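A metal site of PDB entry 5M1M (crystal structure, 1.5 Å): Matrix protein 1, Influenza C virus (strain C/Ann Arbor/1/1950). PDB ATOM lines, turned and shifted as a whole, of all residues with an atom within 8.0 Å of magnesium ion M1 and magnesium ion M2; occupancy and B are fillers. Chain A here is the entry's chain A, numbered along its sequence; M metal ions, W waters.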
ATOM      1  N   ALA A  75       0.656  -7.354  -4.912  1.00  0.00           N
ATOM      2  CA  ALA A  75      -0.319  -7.763  -5.926  1.00  0.00           C
ATOM      3  C   ALA A  75      -1.230  -8.854  -5.380  1.00  0.00           C
ATOM      4  O   ALA A  75      -2.454  -8.819  -5.578  1.00  0.00           O
ATOM      5  CB  ALA A  75       0.403  -8.260  -7.163  1.00  0.00           C
ATOM      6  N   SER A  76      -0.617  -9.809  -4.687  1.00  0.00           N
ATOM      7  CA  SER A  76      -1.345 -10.922  -4.080  1.00  0.00           C
ATOM      8  C   SER A  76      -2.405 -10.414  -3.106  1.00  0.00           C
ATOM      9  O   SER A  76      -3.583 -10.778  -3.211  1.00  0.00           O
ATOM     10  CB  SER A  76      -0.380 -11.854  -3.349  1.00  0.00           C
ATOM     11  OG  SER A  76       0.461 -12.538  -4.271  1.00  0.00           O
ATOM     12  N   ASP A  77      -1.996  -9.561  -2.183  1.00  0.00           N
ATOM     13  CA  ASP A  77      -2.903  -9.021  -1.165  1.00  0.00           C
ATOM     14  C   ASP A  77      -4.021  -8.223  -1.826  1.00  0.00           C
ATOM     15  O   ASP A  77      -5.169  -8.315  -1.397  1.00  0.00           O
ATOM     16  CB  ASP A  77      -2.133  -8.132  -0.167  1.00  0.00           C
ATOM     17  CG  ASP A  77      -1.278  -8.941   0.796  1.00  0.00           C
ATOM     18  OD1 ASP A  77      -1.468 -10.162   0.904  1.00  0.00           O
ATOM     19  OD2 ASP A  77      -0.402  -8.324   1.453  1.00  0.00           O
ATOM     20  N   MET A  78      -3.722  -7.425  -2.813  1.00  0.00           N
ATOM     21  CA  MET A  78      -4.675  -6.678  -3.539  1.00  0.00           C
ATOM     22  C   MET A  78      -5.798  -7.548  -4.131  1.00  0.00           C
ATOM     23  O   MET A  78      -6.940  -7.224  -4.000  1.00  0.00           O
ATOM     24  CB  MET A  78      -3.969  -5.891  -4.616  1.00  0.00           C
ATOM     25  CG  MET A  78      -4.758  -5.063  -5.602  1.00  0.00           C
ATOM     26  SD  MET A  78      -5.626  -5.874  -6.965  1.00  0.00           S
ATOM     27  CE  MET A  78      -4.323  -5.989  -8.193  1.00  0.00           C
ATOM     28  N   LEU A  79      -5.425  -8.626  -4.771  1.00  0.00           N
ATOM     29  CA  LEU A  79      -6.420  -9.523  -5.369  1.00  0.00           C
ATOM     30  C   LEU A  79      -7.285 -10.201  -4.308  1.00  0.00           C
ATOM     31  O   LEU A  79      -8.470 -10.471  -4.534  1.00  0.00           O
ATOM     32  CB  LEU A  79      -5.729 -10.564  -6.256  1.00  0.00           C
ATOM     33  CG  LEU A  79      -5.067  -9.975  -7.512  1.00  0.00           C
ATOM     34  CD1 LEU A  79      -4.044 -10.926  -8.141  1.00  0.00           C
ATOM     35  CD2 LEU A  79      -6.137  -9.617  -8.524  1.00  0.00           C
ATOM     36  N   ASN A  80      -6.694 -10.472  -3.142  1.00  0.00           N
ATOM     37  CA  ASN A  80      -7.431 -11.020  -2.009  1.00  0.00           C
ATOM     38  C   ASN A  80      -8.530 -10.074  -1.526  1.00  0.00           C
ATOM     39  O   ASN A  80      -9.683 -10.468  -1.397  1.00  0.00           O
ATOM     40  CB  ASN A  80      -6.476 -11.311  -0.846  1.00  0.00           C
ATOM     41  CG  ASN A  80      -5.563 -12.481  -1.105  1.00  0.00           C
ATOM     42  OD1 ASN A  80      -5.798 -13.273  -2.037  1.00  0.00           O
ATOM     43  ND2 ASN A  80      -4.530 -12.629  -0.287  1.00  0.00           N
ATOM     44  N   LYS A  81      -8.170  -8.839  -1.287  1.00  0.00           N
ATOM     45  CA  LYS A  81      -9.114  -7.862  -0.812  1.00  0.00           C
ATOM     46  C   LYS A  81     -10.206  -7.613  -1.870  1.00  0.00           C
ATOM     47  O   LYS A  81     -11.377  -7.505  -1.526  1.00  0.00           O
ATOM     48  CB  LYS A  81      -8.367  -6.586  -0.439  1.00  0.00           C
ATOM     49  CG  LYS A  81      -7.532  -6.760   0.798  1.00  0.00           C
ATOM     50  CD  LYS A  81      -8.356  -7.027   2.031  1.00  0.00           C
ATOM     51  CE  LYS A  81      -7.505  -7.497   3.166  1.00  0.00           C
ATOM     52  NZ  LYS A  81      -6.969  -6.398   4.008  1.00  0.00           N
ATOM     53  N   ALA A  82      -9.819  -7.535  -3.129  1.00  0.00           N
ATOM     54  CA  ALA A  82     -10.747  -7.254  -4.231  1.00  0.00           C
ATOM     55  C   ALA A  82     -11.779  -8.361  -4.463  1.00  0.00           C
ATOM     56  O   ALA A  82     -12.773  -8.143  -5.171  1.00  0.00           O
ATOM     57  CB  ALA A  82      -9.976  -7.015  -5.496  1.00  0.00           C
ATOM     58  N   THR A  83     -11.543  -9.534  -3.893  1.00  0.00           N
ATOM     59  CA  THR A  83     -12.474 -10.652  -4.074  1.00  0.00           C
ATOM     60  C   THR A  83     -12.940 -11.236  -2.737  1.00  0.00           C
ATOM     61  O   THR A  83     -13.444 -12.346  -2.686  1.00  0.00           O
ATOM     62  CB  THR A  83     -11.847 -11.781  -4.927  1.00  0.00           C
ATOM     63  OG1 THR A  83     -10.724 -12.343  -4.230  1.00  0.00           O
ATOM     64  CG2 THR A  83     -11.397 -11.262  -6.264  1.00  0.00           C
ATOM     65  N   SER A  84     -12.782 -10.464  -1.659  1.00  0.00           N
ATOM     66  CA  SER A  84     -13.044 -11.000  -0.321  1.00  0.00           C
ATOM     67  C   SER A  84     -14.514 -11.282  -0.035  1.00  0.00           C
ATOM     68  O   SER A  84     -14.835 -12.012   0.897  1.00  0.00           O
ATOM     69  CB  SER A  84     -12.472 -10.060   0.750  1.00  0.00           C
ATOM     70  OG  SER A  84     -13.177  -8.837   0.788  1.00  0.00           O
ATOM     71  N   SER A  85     -15.415 -10.746  -0.869  1.00  0.00           N
ATOM     72  CA  SER A  85     -16.848 -10.949  -0.668  1.00  0.00           C
ATOM     73  C   SER A  85     -17.416 -12.138  -1.444  1.00  0.00           C
ATOM     74  O   SER A  85     -18.618 -12.399  -1.402  1.00  0.00           O
ATOM     75  CB  SER A  85     -17.621  -9.681  -1.026  1.00  0.00           C
ATOM     76  OG  SER A  85     -17.237  -8.600  -0.192  1.00  0.00           O
ATOM     77  N   LEU A  86     -16.550 -12.866  -2.167  1.00  0.00           N
ATOM     78  CA  LEU A  86     -17.003 -14.040  -2.908  1.00  0.00           C
ATOM     79  C   LEU A  86     -17.095 -15.285  -2.043  1.00  0.00           C
ATOM     80  O   LEU A  86     -16.165 -15.600  -1.306  1.00  0.00           O
ATOM     81  CB  LEU A  86     -16.081 -14.323  -4.097  1.00  0.00           C
ATOM     82  CG  LEU A  86     -16.203 -13.385  -5.294  1.00  0.00           C
ATOM     83  CD1 LEU A  86     -15.211 -13.740  -6.371  1.00  0.00           C
ATOM     84  CD2 LEU A  86     -17.609 -13.431  -5.853  1.00  0.00           C
ATOM     85  N   LYS A  87     -18.218 -16.007  -2.148  1.00  0.00           N
ATOM     86  CA  LYS A  87     -18.318 -17.315  -1.520  1.00  0.00           C
ATOM     87  C   LYS A  87     -17.401 -18.294  -2.254  1.00  0.00           C
ATOM     88  O   LYS A  87     -17.139 -18.128  -3.449  1.00  0.00           O
ATOM     89  CB  LYS A  87     -19.766 -17.823  -1.546  1.00  0.00           C
ATOM     90  CG  LYS A  87     -20.706 -16.986  -0.683  1.00  0.00           C
ATOM     91  CD  LYS A  87     -22.170 -17.291  -0.941  1.00  0.00           C
ATOM     92  CE  LYS A  87     -22.553 -18.665  -0.444  1.00  0.00           C
ATOM     93  NZ  LYS A  87     -23.902 -18.642   0.178  1.00  0.00           N
ATOM     94  N   GLY A  91     -16.489 -18.991  -6.453  1.00  0.00           N
ATOM     95  CA  GLY A  91     -15.171 -19.131  -7.042  1.00  0.00           C
ATOM     96  C   GLY A  91     -14.994 -20.468  -7.736  1.00  0.00           C
ATOM     97  O   GLY A  91     -14.332 -20.565  -8.766  1.00  0.00           O
ATOM     98  N   ARG A  95     -13.767 -21.080 -11.532  1.00  0.00           N
ATOM     99  CA  ARG A  95     -12.657 -21.937 -11.960  1.00  0.00           C
ATOM    100  C   ARG A  95     -13.069 -22.869 -13.094  1.00  0.00           C
ATOM    101  O   ARG A  95     -12.359 -22.996 -14.099  1.00  0.00           O
ATOM    102  CB  ARG A  95     -12.086 -22.730 -10.779  1.00  0.00           C
ATOM    103  CG  ARG A  95     -11.394 -21.839  -9.758  1.00  0.00           C
ATOM    104  CD  ARG A  95     -10.550 -22.654  -8.789  1.00  0.00           C
ATOM    105  NE  ARG A  95     -11.326 -23.553  -7.935  1.00  0.00           N
ATOM    106  CZ  ARG A  95     -11.956 -23.182  -6.823  1.00  0.00           C
ATOM    107  NH1 ARG A  95     -11.957 -21.916  -6.434  1.00  0.00           N
ATOM    108  NH2 ARG A  95     -12.615 -24.072  -6.102  1.00  0.00           N
ATOM    109  N   ASP A 119     -15.743  -7.947  -9.153  1.00  0.00           N
ATOM    110  CA  ASP A 119     -15.115  -8.906  -8.233  1.00  0.00           C
ATOM    111  C   ASP A 119     -14.973 -10.316  -8.850  1.00  0.00           C
ATOM    112  O   ASP A 119     -14.031 -11.047  -8.529  1.00  0.00           O
ATOM    113  CB  ASP A 119     -15.805  -8.929  -6.856  1.00  0.00           C
ATOM    114  CG  ASP A 119     -17.232  -9.464  -6.873  1.00  0.00           C
ATOM    115  OD1 ASP A 119     -17.919  -9.433  -7.921  1.00  0.00           O
ATOM    116  OD2 ASP A 119     -17.680  -9.922  -5.804  1.00  0.00           O
ATOM    117  N   MET A 122     -12.191 -10.267 -11.215  1.00  0.00           N
ATOM    118  CA  MET A 122     -10.943 -10.182 -10.496  1.00  0.00           C
ATOM    119  C   MET A 122     -10.513 -11.479  -9.839  1.00  0.00           C
ATOM    120  O   MET A 122      -9.354 -11.719  -9.654  1.00  0.00           O
ATOM    121  CB  MET A 122     -10.992  -9.004  -9.490  1.00  0.00           C
ATOM    122  CG  MET A 122     -11.093  -7.588 -10.167  1.00  0.00           C
ATOM    123  SD  MET A 122      -9.620  -7.359 -11.221  1.00  0.00           S
ATOM    124  CE  MET A 122      -8.568  -7.316  -9.844  1.00  0.00           C
ATOM    125  N   GLU A 123     -11.543 -12.254  -9.562  1.00  0.00           N
ATOM    126  CA  GLU A 123     -11.301 -13.622  -9.122  1.00  0.00           C
ATOM    127  C   GLU A 123     -10.672 -14.485 -10.219  1.00  0.00           C
ATOM    128  O   GLU A 123      -9.865 -15.370  -9.938  1.00  0.00           O
ATOM    129  CB  GLU A 123     -12.623 -14.225  -8.640  1.00  0.00           C
ATOM    130  CG  GLU A 123     -12.517 -15.658  -8.099  1.00  0.00           C
ATOM    131  CD  GLU A 123     -11.913 -15.760  -6.706  1.00  0.00           C
ATOM    132  OE1 GLU A 123     -11.517 -14.727  -6.105  1.00  0.00           O
ATOM    133  OE2 GLU A 123     -11.844 -16.894  -6.180  1.00  0.00           O
ATOM    134  N   MET A 124     -11.043 -14.223 -11.473  1.00  0.00           N
ATOM    135  CA  MET A 124     -10.387 -14.878 -12.612  1.00  0.00           C
ATOM    136  C   MET A 124      -8.912 -14.469 -12.666  1.00  0.00           C
ATOM    137  O   MET A 124      -8.020 -15.311 -12.851  1.00  0.00           O
ATOM    138  CB  MET A 124     -11.069 -14.513 -13.930  1.00  0.00           C
ATOM    139  CG  MET A 124     -12.524 -14.982 -14.017  1.00  0.00           C
ATOM    140  SD  MET A 124     -13.323 -14.317 -15.489  1.00  0.00           S
ATOM    141  CE  MET A 124     -12.473 -15.238 -16.747  1.00  0.00           C
ATOM    142  N   GLU A 126      -7.126 -13.384 -10.147  1.00  0.00           N
ATOM    143  CA  GLU A 126      -6.485 -13.968  -8.974  1.00  0.00           C
ATOM    144  C   GLU A 126      -6.169 -15.442  -9.201  1.00  0.00           C
ATOM    145  O   GLU A 126      -5.113 -15.939  -8.785  1.00  0.00           O
ATOM    146  CB  GLU A 126      -7.366 -13.842  -7.741  1.00  0.00           C
ATOM    147  CG  GLU A 126      -6.650 -14.303  -6.487  1.00  0.00           C
ATOM    148  CD  GLU A 126      -7.556 -14.339  -5.277  1.00  0.00           C
ATOM    149  OE1 GLU A 126      -8.789 -14.188  -5.431  1.00  0.00           O
ATOM    150  OE2 GLU A 126      -7.018 -14.535  -4.168  1.00  0.00           O
ATOM    151  N   GLU A 127      -7.086 -16.163  -9.829  1.00  0.00           N
ATOM    152  CA  GLU A 127      -6.816 -17.560 -10.184  1.00  0.00           C
ATOM    153  C   GLU A 127      -5.539 -17.707 -11.013  1.00  0.00           C
ATOM    154  O   GLU A 127      -4.683 -18.529 -10.700  1.00  0.00           O
ATOM    155  CB  GLU A 127      -8.028 -18.182 -10.900  1.00  0.00           C
ATOM    156  CG  GLU A 127      -9.053 -18.778  -9.962  1.00  0.00           C
ATOM    157  CD  GLU A 127      -8.464 -19.821  -9.024  1.00  0.00           C
ATOM    158  OE1 GLU A 127      -7.800 -20.763  -9.506  1.00  0.00           O
ATOM    159  OE2 GLU A 127      -8.643 -19.683  -7.790  1.00  0.00           O
ATOM    160  N   TYR A 129      -3.061 -15.486 -11.278  1.00  0.00           N
ATOM    161  CA  TYR A 129      -1.894 -14.960 -10.566  1.00  0.00           C
ATOM    162  C   TYR A 129      -1.456 -15.805  -9.375  1.00  0.00           C
ATOM    163  O   TYR A 129      -0.266 -16.023  -9.155  1.00  0.00           O
ATOM    164  CB  TYR A 129      -2.134 -13.521 -10.098  1.00  0.00           C
ATOM    165  CG  TYR A 129      -0.886 -12.812  -9.588  1.00  0.00           C
ATOM    166  CD1 TYR A 129       0.116 -12.414 -10.462  1.00  0.00           C
ATOM    167  CD2 TYR A 129      -0.720 -12.559  -8.237  1.00  0.00           C
ATOM    168  CE1 TYR A 129       1.254 -11.737  -9.997  1.00  0.00           C
ATOM    169  CE2 TYR A 129       0.420 -11.905  -7.775  1.00  0.00           C
ATOM    170  CZ  TYR A 129       1.391 -11.514  -8.649  1.00  0.00           C
ATOM    171  OH  TYR A 129       2.493 -10.849  -8.162  1.00  0.00           O
ATOM    172  N   ASP A 130      -2.433 -16.307  -8.610  1.00  0.00           N
ATOM    173  CA  ASP A 130      -2.149 -17.122  -7.428  1.00  0.00           C
ATOM    174  C   ASP A 130      -1.810 -18.549  -7.841  1.00  0.00           C
ATOM    175  O   ASP A 130      -0.972 -19.202  -7.220  1.00  0.00           O
ATOM    176  CB  ASP A 130      -3.375 -17.179  -6.500  1.00  0.00           C
ATOM    177  CG  ASP A 130      -3.520 -15.939  -5.618  1.00  0.00           C
ATOM    178  OD1 ASP A 130      -2.770 -14.944  -5.791  1.00  0.00           O
ATOM    179  OD2 ASP A 130      -4.432 -15.963  -4.753  1.00  0.00           O
ATOM    180  N   HIS A 131      -2.497 -19.025  -8.871  1.00  0.00           N
ATOM    181  CA  HIS A 131      -2.352 -20.424  -9.304  1.00  0.00           C
ATOM    182  C   HIS A 131      -2.120 -20.594 -10.815  1.00  0.00           C
ATOM    183  O   HIS A 131      -2.849 -21.353 -11.483  1.00  0.00           O
ATOM    184  CB  HIS A 131      -3.584 -21.228  -8.876  1.00  0.00           C
ATOM    185  CG  HIS A 131      -3.924 -21.071  -7.421  1.00  0.00           C
ATOM    186  ND1 HIS A 131      -3.188 -21.653  -6.417  1.00  0.00           N
ATOM    187  CD2 HIS A 131      -4.915 -20.373  -6.808  1.00  0.00           C
ATOM    188  CE1 HIS A 131      -3.704 -21.328  -5.252  1.00  0.00           C
ATOM    189  NE2 HIS A 131      -4.742 -20.556  -5.449  1.00  0.00           N
HETATM  190 MG    MG M   1      -5.136 -14.683  -3.315  1.00  0.00          MG
HETATM  191 MG    MG M   2     -10.407 -14.517  -4.228  1.00  0.00          MG
HETATM  192  O   HOH W   1     -10.205 -16.591  -4.089  1.00  0.00           O
HETATM  193  O   HOH W   2      -5.814 -16.193  -2.148  1.00  0.00           O
HETATM  194  O   HOH W   3      -3.216 -14.932  -2.340  1.00  0.00           O
HETATM  195  O   HOH W   4      -9.125 -14.258  -2.633  1.00  0.00           O
HETATM  196  O   HOH W   5      -4.196 -13.122  -4.466  1.00  0.00           O
HETATM  197  O   HOH W   6     -12.103 -14.583  -3.076  1.00  0.00           O
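The backbone carbonyl oxygen (O) of Leu 79 lies close to the side-chain hydroxyl (OG1) of Thr 83 (2.9 Å).
Of the 24 residues printed, 3 come within 4 Å of magnesium ion M1.
Within 4 Å of magnesium ion M2: Thr 83, Glu 123 and Glu 126.
Magnesium ion M1 is bound by the side-chain amide oxygen (OD1) of Asn 80 (2.0 Å), water W2 (2.0 Å), the side-chain carboxylate (OD2) of Asp 130 (2.0 Å), the side-chain carboxylate (OE2) of Glu 126 (2.1 Å), water W5 (2.2 Å) and water W3 (2.2 Å). Magnesium ion M1 has six donor atoms within binding distance.
Magnesium ion M2 is bound by OE1 of Glu 126 (2.0 Å), water W6 (2.1 Å), water W4 (2.1 Å), water W1 (2.1 Å), OE1 of Glu 123 (2.2 Å) and OG1 of Thr 83 (2.2 Å). Magnesium ion M2 has six donor atoms within binding distance.
Water W5 bridges OD1 of Asp 130 (2.7 Å) and O of Ser 76 (2.7 Å). Water W3 lies within hydrogen-bond range of the side-chain amide nitrogen (ND2) of Asn 80 and the side-chain carboxylate (OD1) of Asp 130.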
